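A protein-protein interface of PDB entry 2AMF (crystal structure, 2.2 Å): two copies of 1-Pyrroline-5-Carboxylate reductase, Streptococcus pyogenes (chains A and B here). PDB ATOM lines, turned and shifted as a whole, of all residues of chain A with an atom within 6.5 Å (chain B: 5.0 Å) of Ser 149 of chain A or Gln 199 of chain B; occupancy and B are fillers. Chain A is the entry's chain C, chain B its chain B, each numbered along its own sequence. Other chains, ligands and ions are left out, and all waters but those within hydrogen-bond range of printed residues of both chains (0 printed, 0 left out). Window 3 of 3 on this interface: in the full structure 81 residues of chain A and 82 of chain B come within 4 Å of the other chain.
NE2 of Gln 199 of chain B lies within hydrogen-bond range of OG of Ser 123 of chain A, 3.1 Å away. OG1 of Thr 200 of chain B sits at hydrogen-bond distance from OG of Ser 123 of chain A (3.1 Å). O of Ala 203 of chain B sits at hydrogen-bond distance from ND2 of Asn 116 of chain A (3.5 Å).
The backbone carbonyl oxygen of Leu 194 of chain B lies within hydrogen-bond range of the side-chain hydroxyl of Thr 198 of chain B (2.6 Å). The backbone carbonyl oxygen (O) of Ile 196 of chain B sits at hydrogen-bond distance from the side-chain hydroxyl (OG1) of Thr 200 of chain B, at 2.9 Å. The backbone NH (N) of Gln 121 of chain A sits at hydrogen-bond distance from the backbone carbonyl oxygen (O) of Asn 116 of chain A. The backbone carbonyl oxygen of Phe 147 of chain A is in hydrogen-bond range of the backbone NH of Ser 122 of chain A, 3.0 Å away. The backbone carbonyl oxygen of Ser 122 of chain A lies within hydrogen-bond range of the backbone NH of Ser 149 of chain A (2.8 Å). N of Thr 124 of chain A is in hydrogen-bond range of O of Ser 149 of chain A, 3.0 Å away.
Among the printed residues, pairs that only touch across the chains: Gln 121 of chain A with Ala 203 of chain B, Phe 151 of chain A with Gln 199 of chain B, Ser 149 of chain A with Gln 199 of chain B, Ala 205 of chain A with Thr 198 of chain B, Ala 205 of chain A with Leu 202 of chain B, Lys 209 of chain A with Leu 202 of chain B, Asn 116 of chain A with Thr 200 of chain B, Phe 151 of chain A with Ile 196 of chain B, Ala 205 of chain A with Val 201 of chain B and Ser 122 of chain A with Gln 199 of chain B.
Of the printed residues of chain B, Asn 116 of chain A touches Thr 200 (3.8 Å) and Ala 203 (3.4 Å). Printed residues of chain B within 4 Å of Gln 121 of chain A: Ala 203 (3.3 Å). Ser 149 of chain A touches just one residue of chain B: Gln 199 (3.3 Å). Leu 194 of chain B touches none of the printed residues of chain A. Val 197 of chain B touches none of the printed residues of chain A. Gln 199 of chain B touches four residues of chain A. The nearest printed residue of chain B that does not touch Ser 149 of chain A is Glu 195 of chain B (7.8 Å). The nearest residue of chain A that does not touch Gln 199 of chain B is Gln 121 of chain A (5.1 Å). The nearest printed residue of chain A that does not touch Ala 203 of chain B is Ser 122 of chain A (5.4 Å).
Of the 10 printed residues of chain B, 7 touch a printed residue of chain A. Hydrophobic or aromatic side chains of chain B that line the printed part of chain A: Ile 196, Val 201, Leu 202 and Ala 203. Of the 17 printed residues of chain A, 8 touch a printed residue of chain B. Hydrophobic or aromatic side chains of chain A within 4 Å of the printed part of chain B: Phe 151 and Ala 205. Among the printed residues, 13 pairs touch across the chains.
No position is printed for both chains. Of the 13 pairs that touch across the chains among the printed residues, none has its exchanged pair printed and touching as well.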
ATOM      1  N   ASN A 116      -1.925  -6.871 -23.317  1.00  0.00           N
ATOM      2  CA  ASN A 116      -1.241  -5.834 -22.529  1.00  0.00           C
ATOM      3  C   ASN A 116      -1.802  -5.675 -21.111  1.00  0.00           C
ATOM      4  O   ASN A 116      -1.250  -4.929 -20.281  1.00  0.00           O
ATOM      5  CB  ASN A 116      -1.206  -4.497 -23.276  1.00  0.00           C
ATOM      6  CG  ASN A 116      -0.500  -4.599 -24.613  1.00  0.00           C
ATOM      7  OD1 ASN A 116      -0.932  -4.012 -25.608  1.00  0.00           O
ATOM      8  ND2 ASN A 116       0.578  -5.373 -24.654  1.00  0.00           N
ATOM      9  N   LEU A 120      -0.697  -4.374 -17.139  1.00  0.00           N
ATOM     10  CA  LEU A 120      -1.784  -3.463 -16.736  1.00  0.00           C
ATOM     11  C   LEU A 120      -1.992  -2.275 -17.706  1.00  0.00           C
ATOM     12  O   LEU A 120      -2.313  -1.155 -17.280  1.00  0.00           O
ATOM     13  CB  LEU A 120      -1.589  -2.974 -15.286  1.00  0.00           C
ATOM     14  CG  LEU A 120      -1.148  -3.974 -14.194  1.00  0.00           C
ATOM     15  CD1 LEU A 120      -1.088  -3.280 -12.811  1.00  0.00           C
ATOM     16  CD2 LEU A 120      -2.012  -5.246 -14.128  1.00  0.00           C
ATOM     17  N   GLN A 121      -1.824  -2.519 -19.012  1.00  0.00           N
ATOM     18  CA  GLN A 121      -2.006  -1.464 -20.006  1.00  0.00           C
ATOM     19  C   GLN A 121      -2.901  -1.863 -21.196  1.00  0.00           C
ATOM     20  O   GLN A 121      -2.685  -1.421 -22.332  1.00  0.00           O
ATOM     21  CB  GLN A 121      -0.646  -0.964 -20.504  1.00  0.00           C
ATOM     22  CG  GLN A 121       0.161  -0.194 -19.461  1.00  0.00           C
ATOM     23  CD  GLN A 121       1.486   0.307 -20.015  1.00  0.00           C
ATOM     24  OE1 GLN A 121       2.530   0.138 -19.382  1.00  0.00           O
ATOM     25  NE2 GLN A 121       1.453   0.912 -21.212  1.00  0.00           N
ATOM     26  N   SER A 122      -3.929  -2.662 -20.918  1.00  0.00           N
ATOM     27  CA  SER A 122      -4.903  -3.037 -21.929  1.00  0.00           C
ATOM     28  C   SER A 122      -5.672  -1.820 -22.482  1.00  0.00           C
ATOM     29  O   SER A 122      -5.846  -0.815 -21.794  1.00  0.00           O
ATOM     30  CB  SER A 122      -5.877  -4.046 -21.331  1.00  0.00           C
ATOM     31  OG  SER A 122      -6.840  -4.411 -22.287  1.00  0.00           O
ATOM     32  N   SER A 123      -6.095  -1.904 -23.736  1.00  0.00           N
ATOM     33  CA  SER A 123      -7.044  -0.937 -24.274  1.00  0.00           C
ATOM     34  C   SER A 123      -8.372  -1.670 -24.349  1.00  0.00           C
ATOM     35  O   SER A 123      -8.624  -2.398 -25.307  1.00  0.00           O
ATOM     36  CB  SER A 123      -6.598  -0.439 -25.651  1.00  0.00           C
ATOM     37  OG  SER A 123      -5.261   0.032 -25.582  1.00  0.00           O
ATOM     38  N   THR A 124      -9.207  -1.486 -23.331  1.00  0.00           N
ATOM     39  CA  THR A 124     -10.373  -2.346 -23.117  1.00  0.00           C
ATOM     40  C   THR A 124     -11.704  -1.644 -23.417  1.00  0.00           C
ATOM     41  O   THR A 124     -12.051  -0.627 -22.783  1.00  0.00           O
ATOM     42  CB  THR A 124     -10.406  -2.897 -21.672  1.00  0.00           C
ATOM     43  OG1 THR A 124      -9.118  -3.414 -21.321  1.00  0.00           O
ATOM     44  CG2 THR A 124     -11.460  -4.009 -21.509  1.00  0.00           C
ATOM     45  N   ALA A 125     -12.452  -2.208 -24.365  1.00  0.00           N
ATOM     46  CA  ALA A 125     -13.804  -1.739 -24.654  1.00  0.00           C
ATOM     47  C   ALA A 125     -14.765  -2.287 -23.616  1.00  0.00           C
ATOM     48  O   ALA A 125     -14.602  -3.409 -23.135  1.00  0.00           O
ATOM     49  CB  ALA A 125     -14.253  -2.160 -26.074  1.00  0.00           C
ATOM     50  N   THR A 144     -12.057  -2.624 -15.062  1.00  0.00           N
ATOM     51  CA  THR A 144     -11.301  -2.592 -16.313  1.00  0.00           C
ATOM     52  C   THR A 144     -10.126  -1.598 -16.224  1.00  0.00           C
ATOM     53  O   THR A 144      -9.037  -1.869 -16.750  1.00  0.00           O
ATOM     54  CB  THR A 144     -12.195  -2.343 -17.579  1.00  0.00           C
ATOM     55  OG1 THR A 144     -12.874  -1.086 -17.470  1.00  0.00           O
ATOM     56  CG2 THR A 144     -13.223  -3.471 -17.767  1.00  0.00           C
ATOM     57  N   ASP A 145     -10.327  -0.480 -15.521  1.00  0.00           N
ATOM     58  CA  ASP A 145      -9.238   0.483 -15.295  1.00  0.00           C
ATOM     59  C   ASP A 145      -8.066  -0.129 -14.520  1.00  0.00           C
ATOM     60  O   ASP A 145      -6.937   0.386 -14.580  1.00  0.00           O
ATOM     61  CB  ASP A 145      -9.737   1.765 -14.600  1.00  0.00           C
ATOM     62  CG  ASP A 145     -10.415   2.748 -15.572  1.00  0.00           C
ATOM     63  OD1 ASP A 145     -10.406   2.512 -16.818  1.00  0.00           O
ATOM     64  OD2 ASP A 145     -10.959   3.764 -15.077  1.00  0.00           O
ATOM     65  N   SER A 146      -8.326  -1.244 -13.832  1.00  0.00           N
ATOM     66  CA  SER A 146      -7.307  -1.872 -12.989  1.00  0.00           C
ATOM     67  C   SER A 146      -6.213  -2.549 -13.804  1.00  0.00           C
ATOM     68  O   SER A 146      -5.077  -2.652 -13.342  1.00  0.00           O
ATOM     69  CB  SER A 146      -7.926  -2.858 -11.990  1.00  0.00           C
ATOM     70  OG  SER A 146      -8.121  -4.149 -12.555  1.00  0.00           O
ATOM     71  N   PHE A 147      -6.553  -3.010 -15.009  1.00  0.00           N
ATOM     72  CA  PHE A 147      -5.590  -3.695 -15.870  1.00  0.00           C
ATOM     73  C   PHE A 147      -5.364  -2.975 -17.209  1.00  0.00           C
ATOM     74  O   PHE A 147      -4.870  -3.568 -18.163  1.00  0.00           O
ATOM     75  CB  PHE A 147      -5.973  -5.174 -16.056  1.00  0.00           C
ATOM     76  CG  PHE A 147      -7.330  -5.388 -16.691  1.00  0.00           C
ATOM     77  CD1 PHE A 147      -7.502  -5.273 -18.079  1.00  0.00           C
ATOM     78  CD2 PHE A 147      -8.429  -5.712 -15.908  1.00  0.00           C
ATOM     79  CE1 PHE A 147      -8.747  -5.474 -18.678  1.00  0.00           C
ATOM     80  CE2 PHE A 147      -9.698  -5.907 -16.484  1.00  0.00           C
ATOM     81  CZ  PHE A 147      -9.856  -5.796 -17.876  1.00  0.00           C
ATOM     82  N   GLY A 148      -5.715  -1.689 -17.260  1.00  0.00           N
ATOM     83  CA  GLY A 148      -5.449  -0.834 -18.412  1.00  0.00           C
ATOM     84  C   GLY A 148      -6.362   0.378 -18.449  1.00  0.00           C
ATOM     85  O   GLY A 148      -6.762   0.879 -17.401  1.00  0.00           O
ATOM     86  N   SER A 149      -6.684   0.844 -19.657  1.00  0.00           N
ATOM     87  CA  SER A 149      -7.664   1.901 -19.867  1.00  0.00           C
ATOM     88  C   SER A 149      -9.008   1.316 -20.330  1.00  0.00           C
ATOM     89  O   SER A 149      -9.087   0.148 -20.773  1.00  0.00           O
ATOM     90  CB  SER A 149      -7.169   2.910 -20.913  1.00  0.00           C
ATOM     91  OG  SER A 149      -6.048   3.654 -20.451  1.00  0.00           O
ATOM     92  N   THR A 150     -10.052   2.140 -20.244  1.00  0.00           N
ATOM     93  CA  THR A 150     -11.407   1.727 -20.614  1.00  0.00           C
ATOM     94  C   THR A 150     -11.988   2.673 -21.641  1.00  0.00           C
ATOM     95  O   THR A 150     -11.855   3.894 -21.507  1.00  0.00           O
ATOM     96  CB  THR A 150     -12.329   1.672 -19.395  1.00  0.00           C
ATOM     97  OG1 THR A 150     -11.738   0.829 -18.392  1.00  0.00           O
ATOM     98  CG2 THR A 150     -13.701   1.135 -19.776  1.00  0.00           C
ATOM     99  N   PHE A 151     -12.629   2.098 -22.666  1.00  0.00           N
ATOM    100  CA  PHE A 151     -13.308   2.862 -23.709  1.00  0.00           C
ATOM    101  C   PHE A 151     -14.821   2.549 -23.705  1.00  0.00           C
ATOM    102  O   PHE A 151     -15.218   1.377 -23.670  1.00  0.00           O
ATOM    103  CB  PHE A 151     -12.698   2.550 -25.082  1.00  0.00           C
ATOM    104  CG  PHE A 151     -11.274   3.014 -25.239  1.00  0.00           C
ATOM    105  CD1 PHE A 151     -10.993   4.224 -25.879  1.00  0.00           C
ATOM    106  CD2 PHE A 151     -10.213   2.250 -24.733  1.00  0.00           C
ATOM    107  CE1 PHE A 151      -9.668   4.677 -26.011  1.00  0.00           C
ATOM    108  CE2 PHE A 151      -8.879   2.683 -24.856  1.00  0.00           C
ATOM    109  CZ  PHE A 151      -8.599   3.900 -25.494  1.00  0.00           C
ATOM    110  N   ALA A 205       5.324   6.344 -31.171  1.00  0.00           N
ATOM    111  CA  ALA A 205       3.929   6.325 -30.712  1.00  0.00           C
ATOM    112  C   ALA A 205       3.703   7.394 -29.610  1.00  0.00           C
ATOM    113  O   ALA A 205       2.670   8.077 -29.562  1.00  0.00           O
ATOM    114  CB  ALA A 205       3.551   4.930 -30.230  1.00  0.00           C
ATOM    115  N   LYS A 209       1.119  10.605 -29.807  1.00  0.00           N
ATOM    116  CA  LYS A 209       0.157  10.833 -28.720  1.00  0.00           C
ATOM    117  C   LYS A 209       0.133  12.268 -28.146  1.00  0.00           C
ATOM    118  O   LYS A 209      -0.928  12.807 -27.865  1.00  0.00           O
ATOM    119  CB  LYS A 209       0.438   9.845 -27.578  1.00  0.00           C
ATOM    120  CG  LYS A 209      -0.692   9.699 -26.578  1.00  0.00           C
ATOM    121  CD  LYS A 209      -0.337   8.705 -25.494  1.00  0.00           C
ATOM    122  CE  LYS A 209       0.173   9.411 -24.225  1.00  0.00           C
ATOM    123  NZ  LYS A 209       1.385   8.733 -23.628  1.00  0.00           N
ATOM    124  N   LEU B 194      -7.330   6.377 -34.102  1.00  0.00           N
ATOM    125  CA  LEU B 194      -5.924   6.740 -33.835  1.00  0.00           C
ATOM    126  C   LEU B 194      -5.574   6.659 -32.346  1.00  0.00           C
ATOM    127  O   LEU B 194      -4.471   6.260 -31.994  1.00  0.00           O
ATOM    128  CB  LEU B 194      -5.587   8.144 -34.342  1.00  0.00           C
ATOM    129  CG  LEU B 194      -5.147   8.274 -35.796  1.00  0.00           C
ATOM    130  CD1 LEU B 194      -5.011   9.738 -36.156  1.00  0.00           C
ATOM    131  CD2 LEU B 194      -3.817   7.494 -36.074  1.00  0.00           C
ATOM    132  N   GLU B 195      -6.524   7.020 -31.484  1.00  0.00           N
ATOM    133  CA  GLU B 195      -6.273   7.001 -30.052  1.00  0.00           C
ATOM    134  C   GLU B 195      -6.116   5.558 -29.578  1.00  0.00           C
ATOM    135  O   GLU B 195      -5.206   5.242 -28.825  1.00  0.00           O
ATOM    136  CB  GLU B 195      -7.406   7.705 -29.292  1.00  0.00           C
ATOM    137  CG  GLU B 195      -7.229   7.674 -27.758  1.00  0.00           C
ATOM    138  CD  GLU B 195      -8.338   8.389 -27.006  1.00  0.00           C
ATOM    139  OE1 GLU B 195      -9.480   8.453 -27.523  1.00  0.00           O
ATOM    140  OE2 GLU B 195      -8.059   8.885 -25.883  1.00  0.00           O
ATOM    141  N   ILE B 196      -7.015   4.694 -30.031  1.00  0.00           N
ATOM    142  CA  ILE B 196      -7.028   3.294 -29.634  1.00  0.00           C
ATOM    143  C   ILE B 196      -5.752   2.599 -30.108  1.00  0.00           C
ATOM    144  O   ILE B 196      -5.062   1.971 -29.300  1.00  0.00           O
ATOM    145  CB  ILE B 196      -8.285   2.559 -30.182  1.00  0.00           C
ATOM    146  CG1 ILE B 196      -9.553   3.126 -29.550  1.00  0.00           C
ATOM    147  CG2 ILE B 196      -8.200   1.047 -29.960  1.00  0.00           C
ATOM    148  CD1 ILE B 196     -10.824   2.768 -30.335  1.00  0.00           C
ATOM    149  N   VAL B 197      -5.414   2.717 -31.393  1.00  0.00           N
ATOM    150  CA  VAL B 197      -4.235   1.969 -31.867  1.00  0.00           C
ATOM    151  C   VAL B 197      -2.893   2.495 -31.335  1.00  0.00           C
ATOM    152  O   VAL B 197      -2.022   1.716 -30.950  1.00  0.00           O
ATOM    153  CB  VAL B 197      -4.193   1.663 -33.438  1.00  0.00           C
ATOM    154  CG1 VAL B 197      -5.539   1.616 -34.053  1.00  0.00           C
ATOM    155  CG2 VAL B 197      -3.285   2.600 -34.172  1.00  0.00           C
ATOM    156  N   THR B 198      -2.740   3.816 -31.301  1.00  0.00           N
ATOM    157  CA  THR B 198      -1.537   4.440 -30.759  1.00  0.00           C
ATOM    158  C   THR B 198      -1.267   3.957 -29.317  1.00  0.00           C
ATOM    159  O   THR B 198      -0.114   3.676 -28.936  1.00  0.00           O
ATOM    160  CB  THR B 198      -1.668   5.980 -30.773  1.00  0.00           C
ATOM    161  OG1 THR B 198      -1.834   6.437 -32.131  1.00  0.00           O
ATOM    162  CG2 THR B 198      -0.453   6.629 -30.136  1.00  0.00           C
ATOM    163  N   GLN B 199      -2.336   3.859 -28.535  1.00  0.00           N
ATOM    164  CA  GLN B 199      -2.249   3.425 -27.151  1.00  0.00           C
ATOM    165  C   GLN B 199      -1.919   1.942 -27.083  1.00  0.00           C
ATOM    166  O   GLN B 199      -1.212   1.505 -26.196  1.00  0.00           O
ATOM    167  CB  GLN B 199      -3.583   3.710 -26.437  1.00  0.00           C
ATOM    168  CG  GLN B 199      -3.672   3.134 -25.022  1.00  0.00           C
ATOM    169  CD  GLN B 199      -4.953   3.528 -24.285  1.00  0.00           C
ATOM    170  OE1 GLN B 199      -5.235   4.730 -24.077  1.00  0.00           O
ATOM    171  NE2 GLN B 199      -5.721   2.519 -23.869  1.00  0.00           N
ATOM    172  N   THR B 200      -2.446   1.173 -28.029  1.00  0.00           N
ATOM    173  CA  THR B 200      -2.159  -0.252 -28.144  1.00  0.00           C
ATOM    174  C   THR B 200      -0.721  -0.493 -28.649  1.00  0.00           C
ATOM    175  O   THR B 200      -0.040  -1.399 -28.187  1.00  0.00           O
ATOM    176  CB  THR B 200      -3.230  -0.943 -29.040  1.00  0.00           C
ATOM    177  OG1 THR B 200      -4.523  -0.755 -28.444  1.00  0.00           O
ATOM    178  CG2 THR B 200      -2.954  -2.438 -29.233  1.00  0.00           C
ATOM    179  N   VAL B 201      -0.248   0.325 -29.572  1.00  0.00           N
ATOM    180  CA  VAL B 201       1.167   0.232 -30.007  1.00  0.00           C
ATOM    181  C   VAL B 201       2.087   0.454 -28.792  1.00  0.00           C
ATOM    182  O   VAL B 201       2.951  -0.392 -28.475  1.00  0.00           O
ATOM    183  CB  VAL B 201       1.475   1.217 -31.155  1.00  0.00           C
ATOM    184  CG1 VAL B 201       2.972   1.254 -31.469  1.00  0.00           C
ATOM    185  CG2 VAL B 201       0.691   0.837 -32.434  1.00  0.00           C
ATOM    186  N   LEU B 202       1.846   1.558 -28.085  1.00  0.00           N
ATOM    187  CA  LEU B 202       2.620   1.916 -26.907  1.00  0.00           C
ATOM    188  C   LEU B 202       2.679   0.786 -25.885  1.00  0.00           C
ATOM    189  O   LEU B 202       3.753   0.436 -25.408  1.00  0.00           O
ATOM    190  CB  LEU B 202       2.038   3.166 -26.238  1.00  0.00           C
ATOM    191  CG  LEU B 202       2.523   4.516 -26.761  1.00  0.00           C
ATOM    192  CD1 LEU B 202       1.630   5.619 -26.226  1.00  0.00           C
ATOM    193  CD2 LEU B 202       3.947   4.765 -26.336  1.00  0.00           C
ATOM    194  N   ALA B 203       1.520   0.231 -25.549  1.00  0.00           N
ATOM    195  CA  ALA B 203       1.434  -0.811 -24.550  1.00  0.00           C
ATOM    196  C   ALA B 203       2.119  -2.084 -25.025  1.00  0.00           C
ATOM    197  O   ALA B 203       2.792  -2.751 -24.237  1.00  0.00           O
ATOM    198  CB  ALA B 203      -0.007  -1.085 -24.226  1.00  0.00           C
